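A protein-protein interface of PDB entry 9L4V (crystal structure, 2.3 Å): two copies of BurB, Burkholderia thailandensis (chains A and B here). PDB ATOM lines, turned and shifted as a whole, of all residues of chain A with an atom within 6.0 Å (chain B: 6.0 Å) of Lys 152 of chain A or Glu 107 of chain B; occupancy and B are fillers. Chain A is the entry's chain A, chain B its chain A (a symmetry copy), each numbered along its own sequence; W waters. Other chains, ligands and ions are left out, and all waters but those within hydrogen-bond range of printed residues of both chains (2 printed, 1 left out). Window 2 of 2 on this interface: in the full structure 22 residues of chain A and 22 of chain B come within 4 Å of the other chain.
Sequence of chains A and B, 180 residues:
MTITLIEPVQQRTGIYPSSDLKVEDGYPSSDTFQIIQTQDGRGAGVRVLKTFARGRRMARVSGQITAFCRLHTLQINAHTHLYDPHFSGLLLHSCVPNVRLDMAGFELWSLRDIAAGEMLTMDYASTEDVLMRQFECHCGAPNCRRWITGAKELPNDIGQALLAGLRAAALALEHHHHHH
The side-chain amino group (NZ) of Lys 152 of chain A is in salt-bridge range of the side-chain carboxylate (OD2) of Asp 102 of chain B, at 2.5 Å.
The side-chain amino group of Lys 152 of chain A is in salt-bridge range of the side-chain carboxylate of Glu 107 of chain B (3.4 Å).
The side-chain carboxylate (OE1) of Glu 107 of chain B sits at hydrogen-bond distance from the indole nitrogen (NE1) of Trp 109 of chain B (2.9 Å).
The backbone NH (N) of Arg 100 of chain B is in hydrogen-bond range of the backbone carbonyl oxygen (O) of Trp 109 of chain B (2.8 Å).
The guanidinium group of Arg 57 of chain B is in salt-bridge range of the side-chain carboxylate of Glu 107 of chain B (3.6 Å).
NH1 of Arg 60 of chain B lies within salt-bridge range of OE2 of Glu 107 of chain B (3.4 Å).
OD1 of Asp 129 of chain A lies within salt-bridge range of NZ of Lys 152 of chain A.
The backbone carbonyl oxygen (O) of Glu 107 of chain B is in hydrogen-bond range of the backbone NH (N) of Asp 102 of chain B, at 2.8 Å.
Among the printed residues, merely in contact across the chains: Leu 154 of chain A with Gly 55 of chain B, Lys 152 of chain A with Trp 109 of chain B, Ala 151 of chain A with Trp 109 of chain B, Glu 128 of chain A with Arg 100 of chain B, Ala 151 of chain A with Arg 100 of chain B and Ala 151 of chain A with Gly 55 of chain B.
Of chain B, only Asp 102 (2.5 Å), Glu 107 (3.4 Å) and Trp 109 (3.5 Å) come within 4 Å of Lys 152 of chain A.
Of the printed residues of chain B, Leu 154 of chain A touches Gly 55 (3.3 Å).
Printed residues of chain A within 4 Å of Gly 55 of chain B: Ala 151 (3.95 Å) and Leu 154 (3.3 Å).
Glu 107 of chain B touches one residue of chain A.
The nearest residue of chain B that does not touch Lys 152 of chain A is Gly 55 of chain B (4.7 Å).
Hydrophobic or aromatic side chains of chain B that line the printed part of chain A: Trp 109.
Of the 8 printed residues of chain A, 4 touch a printed residue of chain B.
Hydrophobic or aromatic side chains of chain A that line the printed part of chain B: Ala 151 and Leu 154.
No position is printed for both chains.
Of the 8 pairs that touch across the chains among the printed residues, none has its exchanged pair printed and touching as well.
Water W1 lies within hydrogen-bond range of the backbone carbonyl oxygen (O) of Ala 151 of chain A and the backbone NH (N) of Gly 55 of chain B.
Water W2 bridges the backbone carbonyl oxygen of Glu 153 of chain A and the backbone NH of Gly 55 of chain B.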
ATOM      1  N   GLU A 128      -4.345 -16.057  16.755  1.00  0.00           N
ATOM      2  CA  GLU A 128      -5.714 -16.108  17.265  1.00  0.00           C
ATOM      3  C   GLU A 128      -6.415 -17.391  16.832  1.00  0.00           C
ATOM      4  O   GLU A 128      -6.447 -17.710  15.642  1.00  0.00           O
ATOM      5  CB  GLU A 128      -6.504 -14.891  16.775  1.00  0.00           C
ATOM      6  CG  GLU A 128      -5.774 -13.561  16.984  1.00  0.00           C
ATOM      7  CD  GLU A 128      -5.500 -13.288  18.452  1.00  0.00           C
ATOM      8  OE1 GLU A 128      -6.481 -13.206  19.227  1.00  0.00           O
ATOM      9  OE2 GLU A 128      -4.308 -13.183  18.834  1.00  0.00           O
ATOM     10  N   ASP A 129      -6.976 -18.126  17.801  1.00  0.00           N
ATOM     11  CA  ASP A 129      -7.898 -19.216  17.469  1.00  0.00           C
ATOM     12  C   ASP A 129      -9.168 -18.667  16.811  1.00  0.00           C
ATOM     13  O   ASP A 129      -9.607 -19.161  15.764  1.00  0.00           O
ATOM     14  CB  ASP A 129      -8.297 -19.990  18.734  1.00  0.00           C
ATOM     15  CG  ASP A 129      -7.128 -20.648  19.437  1.00  0.00           C
ATOM     16  OD1 ASP A 129      -6.037 -20.785  18.834  1.00  0.00           O
ATOM     17  OD2 ASP A 129      -7.315 -21.026  20.617  1.00  0.00           O
ATOM     18  N   VAL A 130      -9.783 -17.663  17.443  1.00  0.00           N
ATOM     19  CA  VAL A 130     -11.077 -17.104  17.048  1.00  0.00           C
ATOM     20  C   VAL A 130     -11.000 -15.587  17.212  1.00  0.00           C
ATOM     21  O   VAL A 130     -10.383 -15.087  18.157  1.00  0.00           O
ATOM     22  CB  VAL A 130     -12.237 -17.713  17.883  1.00  0.00           C
ATOM     23  CG1 VAL A 130     -13.582 -17.226  17.396  1.00  0.00           C
ATOM     24  CG2 VAL A 130     -12.246 -19.253  17.783  1.00  0.00           C
ATOM     25  N   GLY A 150     -10.184 -16.309  12.776  1.00  0.00           N
ATOM     26  CA  GLY A 150      -9.136 -16.998  13.492  1.00  0.00           C
ATOM     27  C   GLY A 150      -8.702 -18.251  12.756  1.00  0.00           C
ATOM     28  O   GLY A 150      -9.371 -18.740  11.842  1.00  0.00           O
ATOM     29  N   ALA A 151      -7.559 -18.792  13.166  1.00  0.00           N
ATOM     30  CA  ALA A 151      -7.090 -20.002  12.505  1.00  0.00           C
ATOM     31  C   ALA A 151      -8.032 -21.176  12.756  1.00  0.00           C
ATOM     32  O   ALA A 151      -8.173 -22.046  11.892  1.00  0.00           O
ATOM     33  CB  ALA A 151      -5.673 -20.346  12.963  1.00  0.00           C
ATOM     34  N   LYS A 152      -8.679 -21.222  13.922  1.00  0.00           N
ATOM     35  CA  LYS A 152      -9.526 -22.348  14.302  1.00  0.00           C
ATOM     36  C   LYS A 152     -11.010 -22.026  14.143  1.00  0.00           C
ATOM     37  O   LYS A 152     -11.842 -22.577  14.869  1.00  0.00           O
ATOM     38  CB  LYS A 152      -9.217 -22.784  15.739  1.00  0.00           C
ATOM     39  CG  LYS A 152      -7.723 -23.082  15.970  1.00  0.00           C
ATOM     40  CD  LYS A 152      -7.427 -23.668  17.358  1.00  0.00           C
ATOM     41  CE  LYS A 152      -5.924 -23.945  17.527  1.00  0.00           C
ATOM     42  NZ  LYS A 152      -5.552 -24.549  18.856  1.00  0.00           N
ATOM     43  N   GLU A 153     -11.347 -21.133  13.210  1.00  0.00           N
ATOM     44  CA  GLU A 153     -12.666 -20.519  13.108  1.00  0.00           C
ATOM     45  C   GLU A 153     -13.160 -20.643  11.671  1.00  0.00           C
ATOM     46  O   GLU A 153     -12.475 -20.216  10.735  1.00  0.00           O
ATOM     47  CB  GLU A 153     -12.617 -19.036  13.522  1.00  0.00           C
ATOM     48  CG  GLU A 153     -13.963 -18.302  13.483  1.00  0.00           C
ATOM     49  CD  GLU A 153     -13.881 -16.845  13.969  1.00  0.00           C
ATOM     50  OE1 GLU A 153     -12.761 -16.278  14.004  1.00  0.00           O
ATOM     51  OE2 GLU A 153     -14.941 -16.268  14.322  1.00  0.00           O
ATOM     52  N   LEU A 154     -14.341 -21.234  11.499  1.00  0.00           N
ATOM     53  CA  LEU A 154     -14.940 -21.292  10.170  1.00  0.00           C
ATOM     54  C   LEU A 154     -15.522 -19.925   9.799  1.00  0.00           C
ATOM     55  O   LEU A 154     -16.029 -19.202  10.665  1.00  0.00           O
ATOM     56  CB  LEU A 154     -16.044 -22.353  10.130  1.00  0.00           C
ATOM     57  CG  LEU A 154     -15.640 -23.802  10.429  1.00  0.00           C
ATOM     58  CD1 LEU A 154     -16.892 -24.642  10.695  1.00  0.00           C
ATOM     59  CD2 LEU A 154     -14.851 -24.398   9.270  1.00  0.00           C
ATOM     60  N   GLY B  55     -10.167 -23.587   7.869  1.00  0.00           N
ATOM     61  CA  GLY B  55     -10.674 -23.549   9.224  1.00  0.00           C
ATOM     62  C   GLY B  55     -11.018 -24.888   9.834  1.00  0.00           C
ATOM     63  O   GLY B  55     -11.939 -24.966  10.655  1.00  0.00           O
ATOM     64  N   ARG B  57      -9.360 -28.638  11.669  1.00  0.00           N
ATOM     65  CA  ARG B  57      -8.173 -29.287  12.213  1.00  0.00           C
ATOM     66  C   ARG B  57      -7.767 -30.435  11.298  1.00  0.00           C
ATOM     67  O   ARG B  57      -8.504 -31.419  11.158  1.00  0.00           O
ATOM     68  CB  ARG B  57      -8.432 -29.799  13.623  1.00  0.00           C
ATOM     69  CG  ARG B  57      -7.165 -30.291  14.295  1.00  0.00           C
ATOM     70  CD  ARG B  57      -7.453 -30.840  15.668  1.00  0.00           C
ATOM     71  NE  ARG B  57      -8.012 -32.181  15.592  1.00  0.00           N
ATOM     72  CZ  ARG B  57      -8.621 -32.793  16.600  1.00  0.00           C
ATOM     73  NH1 ARG B  57      -8.766 -32.205  17.780  1.00  0.00           N
ATOM     74  NH2 ARG B  57      -9.103 -34.019  16.420  1.00  0.00           N
ATOM     75  N   ALA B  59      -4.883 -32.298  11.700  1.00  0.00           N
ATOM     76  CA  ALA B  59      -4.172 -33.355  12.415  1.00  0.00           C
ATOM     77  C   ALA B  59      -3.761 -32.865  13.790  1.00  0.00           C
ATOM     78  O   ALA B  59      -3.469 -31.683  13.984  1.00  0.00           O
ATOM     79  CB  ALA B  59      -2.926 -33.829  11.643  1.00  0.00           C
ATOM     80  N   ARG B  60      -3.750 -33.792  14.741  1.00  0.00           N
ATOM     81  CA  ARG B  60      -2.974 -33.596  15.951  1.00  0.00           C
ATOM     82  C   ARG B  60      -1.505 -33.859  15.633  1.00  0.00           C
ATOM     83  O   ARG B  60      -1.173 -34.641  14.735  1.00  0.00           O
ATOM     84  CB  ARG B  60      -3.464 -34.524  17.069  1.00  0.00           C
ATOM     85  CG  ARG B  60      -4.804 -34.112  17.713  1.00  0.00           C
ATOM     86  CD  ARG B  60      -5.073 -34.970  18.974  1.00  0.00           C
ATOM     87  NE  ARG B  60      -6.396 -34.780  19.567  1.00  0.00           N
ATOM     88  CZ  ARG B  60      -6.756 -33.708  20.258  1.00  0.00           C
ATOM     89  NH1 ARG B  60      -5.932 -32.674  20.418  1.00  0.00           N
ATOM     90  NH2 ARG B  60      -7.966 -33.671  20.813  1.00  0.00           N
ATOM     91  N   VAL B  61      -0.620 -33.199  16.373  1.00  0.00           N
ATOM     92  CA  VAL B  61       0.811 -33.282  16.130  1.00  0.00           C
ATOM     93  C   VAL B  61       1.494 -33.842  17.375  1.00  0.00           C
ATOM     94  O   VAL B  61       1.024 -33.643  18.503  1.00  0.00           O
ATOM     95  CB  VAL B  61       1.353 -31.889  15.755  1.00  0.00           C
ATOM     96  CG1 VAL B  61       2.897 -31.845  15.772  1.00  0.00           C
ATOM     97  CG2 VAL B  61       0.786 -31.469  14.393  1.00  0.00           C
ATOM     98  N   ARG B 100      -1.558 -23.605   9.374  1.00  0.00           N
ATOM     99  CA  ARG B 100      -0.880 -23.112  10.571  1.00  0.00           C
ATOM    100  C   ARG B 100      -0.582 -24.292  11.479  1.00  0.00           C
ATOM    101  O   ARG B 100      -1.470 -25.106  11.750  1.00  0.00           O
ATOM    102  CB  ARG B 100      -1.715 -22.089  11.348  1.00  0.00           C
ATOM    103  CG  ARG B 100      -1.183 -21.914  12.809  1.00  0.00           C
ATOM    104  CD  ARG B 100      -1.560 -20.606  13.462  1.00  0.00           C
ATOM    105  NE  ARG B 100      -1.238 -20.622  14.890  1.00  0.00           N
ATOM    106  CZ  ARG B 100      -1.976 -20.036  15.824  1.00  0.00           C
ATOM    107  NH1 ARG B 100      -3.044 -19.330  15.508  1.00  0.00           N
ATOM    108  NH2 ARG B 100      -1.657 -20.196  17.109  1.00  0.00           N
ATOM    109  N   LEU B 101       0.657 -24.385  11.944  1.00  0.00           N
ATOM    110  CA  LEU B 101       1.014 -25.339  12.983  1.00  0.00           C
ATOM    111  C   LEU B 101       0.904 -24.636  14.337  1.00  0.00           C
ATOM    112  O   LEU B 101       1.715 -23.755  14.663  1.00  0.00           O
ATOM    113  CB  LEU B 101       2.421 -25.881  12.762  1.00  0.00           C
ATOM    114  CG  LEU B 101       2.925 -26.841  13.833  1.00  0.00           C
ATOM    115  CD1 LEU B 101       1.977 -28.016  14.055  1.00  0.00           C
ATOM    116  CD2 LEU B 101       4.234 -27.344  13.383  1.00  0.00           C
ATOM    117  N   ASP B 102      -0.124 -24.985  15.102  1.00  0.00           N
ATOM    118  CA  ASP B 102      -0.317 -24.436  16.440  1.00  0.00           C
ATOM    119  C   ASP B 102       0.561 -25.238  17.395  1.00  0.00           C
ATOM    120  O   ASP B 102       0.286 -26.410  17.649  1.00  0.00           O
ATOM    121  CB  ASP B 102      -1.788 -24.508  16.839  1.00  0.00           C
ATOM    122  CG  ASP B 102      -1.996 -24.414  18.344  1.00  0.00           C
ATOM    123  OD1 ASP B 102      -1.121 -23.838  19.057  1.00  0.00           O
ATOM    124  OD2 ASP B 102      -3.043 -24.940  18.807  1.00  0.00           O
ATOM    125  N   MET B 103       1.617 -24.615  17.907  1.00  0.00           N
ATOM    126  CA  MET B 103       2.586 -25.241  18.805  1.00  0.00           C
ATOM    127  C   MET B 103       2.204 -25.155  20.284  1.00  0.00           C
ATOM    128  O   MET B 103       2.999 -25.567  21.142  1.00  0.00           O
ATOM    129  CB  MET B 103       3.968 -24.598  18.594  1.00  0.00           C
ATOM    130  CG  MET B 103       4.805 -25.022  17.391  1.00  0.00           C
ATOM    131  SD  MET B 103       4.588 -26.656  16.678  1.00  0.00           S
ATOM    132  CE  MET B 103       5.828 -27.490  17.695  1.00  0.00           C
ATOM    133  N   GLY B 105      -1.439 -25.932  21.226  1.00  0.00           N
ATOM    134  CA  GLY B 105      -2.345 -27.062  21.180  1.00  0.00           C
ATOM    135  C   GLY B 105      -1.827 -28.268  20.423  1.00  0.00           C
ATOM    136  O   GLY B 105      -2.443 -29.341  20.499  1.00  0.00           O
ATOM    137  N   PHE B 106      -0.698 -28.112  19.717  1.00  0.00           N
ATOM    138  CA  PHE B 106      -0.084 -29.158  18.888  1.00  0.00           C
ATOM    139  C   PHE B 106      -1.098 -29.739  17.897  1.00  0.00           C
ATOM    140  O   PHE B 106      -1.432 -30.931  17.911  1.00  0.00           O
ATOM    141  CB  PHE B 106       0.571 -30.236  19.760  1.00  0.00           C
ATOM    142  CG  PHE B 106       1.757 -29.720  20.539  1.00  0.00           C
ATOM    143  CD1 PHE B 106       1.563 -29.037  21.740  1.00  0.00           C
ATOM    144  CD2 PHE B 106       3.050 -29.887  20.064  1.00  0.00           C
ATOM    145  CE1 PHE B 106       2.632 -28.531  22.468  1.00  0.00           C
ATOM    146  CE2 PHE B 106       4.151 -29.370  20.786  1.00  0.00           C
ATOM    147  CZ  PHE B 106       3.939 -28.699  21.988  1.00  0.00           C
ATOM    148  N   GLU B 107      -1.570 -28.856  17.013  1.00  0.00           N
ATOM    149  CA  GLU B 107      -2.543 -29.190  15.985  1.00  0.00           C
ATOM    150  C   GLU B 107      -2.176 -28.447  14.708  1.00  0.00           C
ATOM    151  O   GLU B 107      -1.649 -27.334  14.751  1.00  0.00           O
ATOM    152  CB  GLU B 107      -3.983 -28.813  16.401  1.00  0.00           C
ATOM    153  CG  GLU B 107      -4.428 -29.356  17.755  1.00  0.00           C
ATOM    154  CD  GLU B 107      -5.822 -28.892  18.165  1.00  0.00           C
ATOM    155  OE1 GLU B 107      -6.214 -27.756  17.801  1.00  0.00           O
ATOM    156  OE2 GLU B 107      -6.516 -29.661  18.879  1.00  0.00           O
ATOM    157  N   LEU B 108      -2.475 -29.067  13.567  1.00  0.00           N
ATOM    158  CA  LEU B 108      -2.316 -28.442  12.260  1.00  0.00           C
ATOM    159  C   LEU B 108      -3.691 -28.014  11.748  1.00  0.00           C
ATOM    160  O   LEU B 108      -4.622 -28.830  11.730  1.00  0.00           O
ATOM    161  CB  LEU B 108      -1.660 -29.434  11.293  1.00  0.00           C
ATOM    162  CG  LEU B 108      -1.262 -28.923   9.918  1.00  0.00           C
ATOM    163  CD1 LEU B 108      -0.078 -27.974  10.074  1.00  0.00           C
ATOM    164  CD2 LEU B 108      -0.935 -30.075   8.955  1.00  0.00           C
ATOM    165  N   TRP B 109      -3.827 -26.742  11.345  1.00  0.00           N
ATOM    166  CA  TRP B 109      -5.109 -26.219  10.858  1.00  0.00           C
ATOM    167  C   TRP B 109      -4.978 -25.596   9.468  1.00  0.00           C
ATOM    168  O   TRP B 109      -3.997 -24.908   9.164  1.00  0.00           O
ATOM    169  CB  TRP B 109      -5.708 -25.159  11.804  1.00  0.00           C
ATOM    170  CG  TRP B 109      -6.235 -25.704  13.112  1.00  0.00           C
ATOM    171  CD1 TRP B 109      -5.487 -26.139  14.177  1.00  0.00           C
ATOM    172  CD2 TRP B 109      -7.612 -25.849  13.501  1.00  0.00           C
ATOM    173  NE1 TRP B 109      -6.318 -26.542  15.205  1.00  0.00           N
ATOM    174  CE2 TRP B 109      -7.623 -26.379  14.816  1.00  0.00           C
ATOM    175  CE3 TRP B 109      -8.835 -25.572  12.875  1.00  0.00           C
ATOM    176  CZ2 TRP B 109      -8.817 -26.654  15.507  1.00  0.00           C
ATOM    177  CZ3 TRP B 109     -10.032 -25.845  13.570  1.00  0.00           C
ATOM    178  CH2 TRP B 109     -10.007 -26.378  14.868  1.00  0.00           C
HETATM  179  O   HOH W   1      -8.276 -21.132   9.215  1.00  0.00           O
HETATM  180  O   HOH W   2     -10.982 -20.496   8.179  1.00  0.00           O
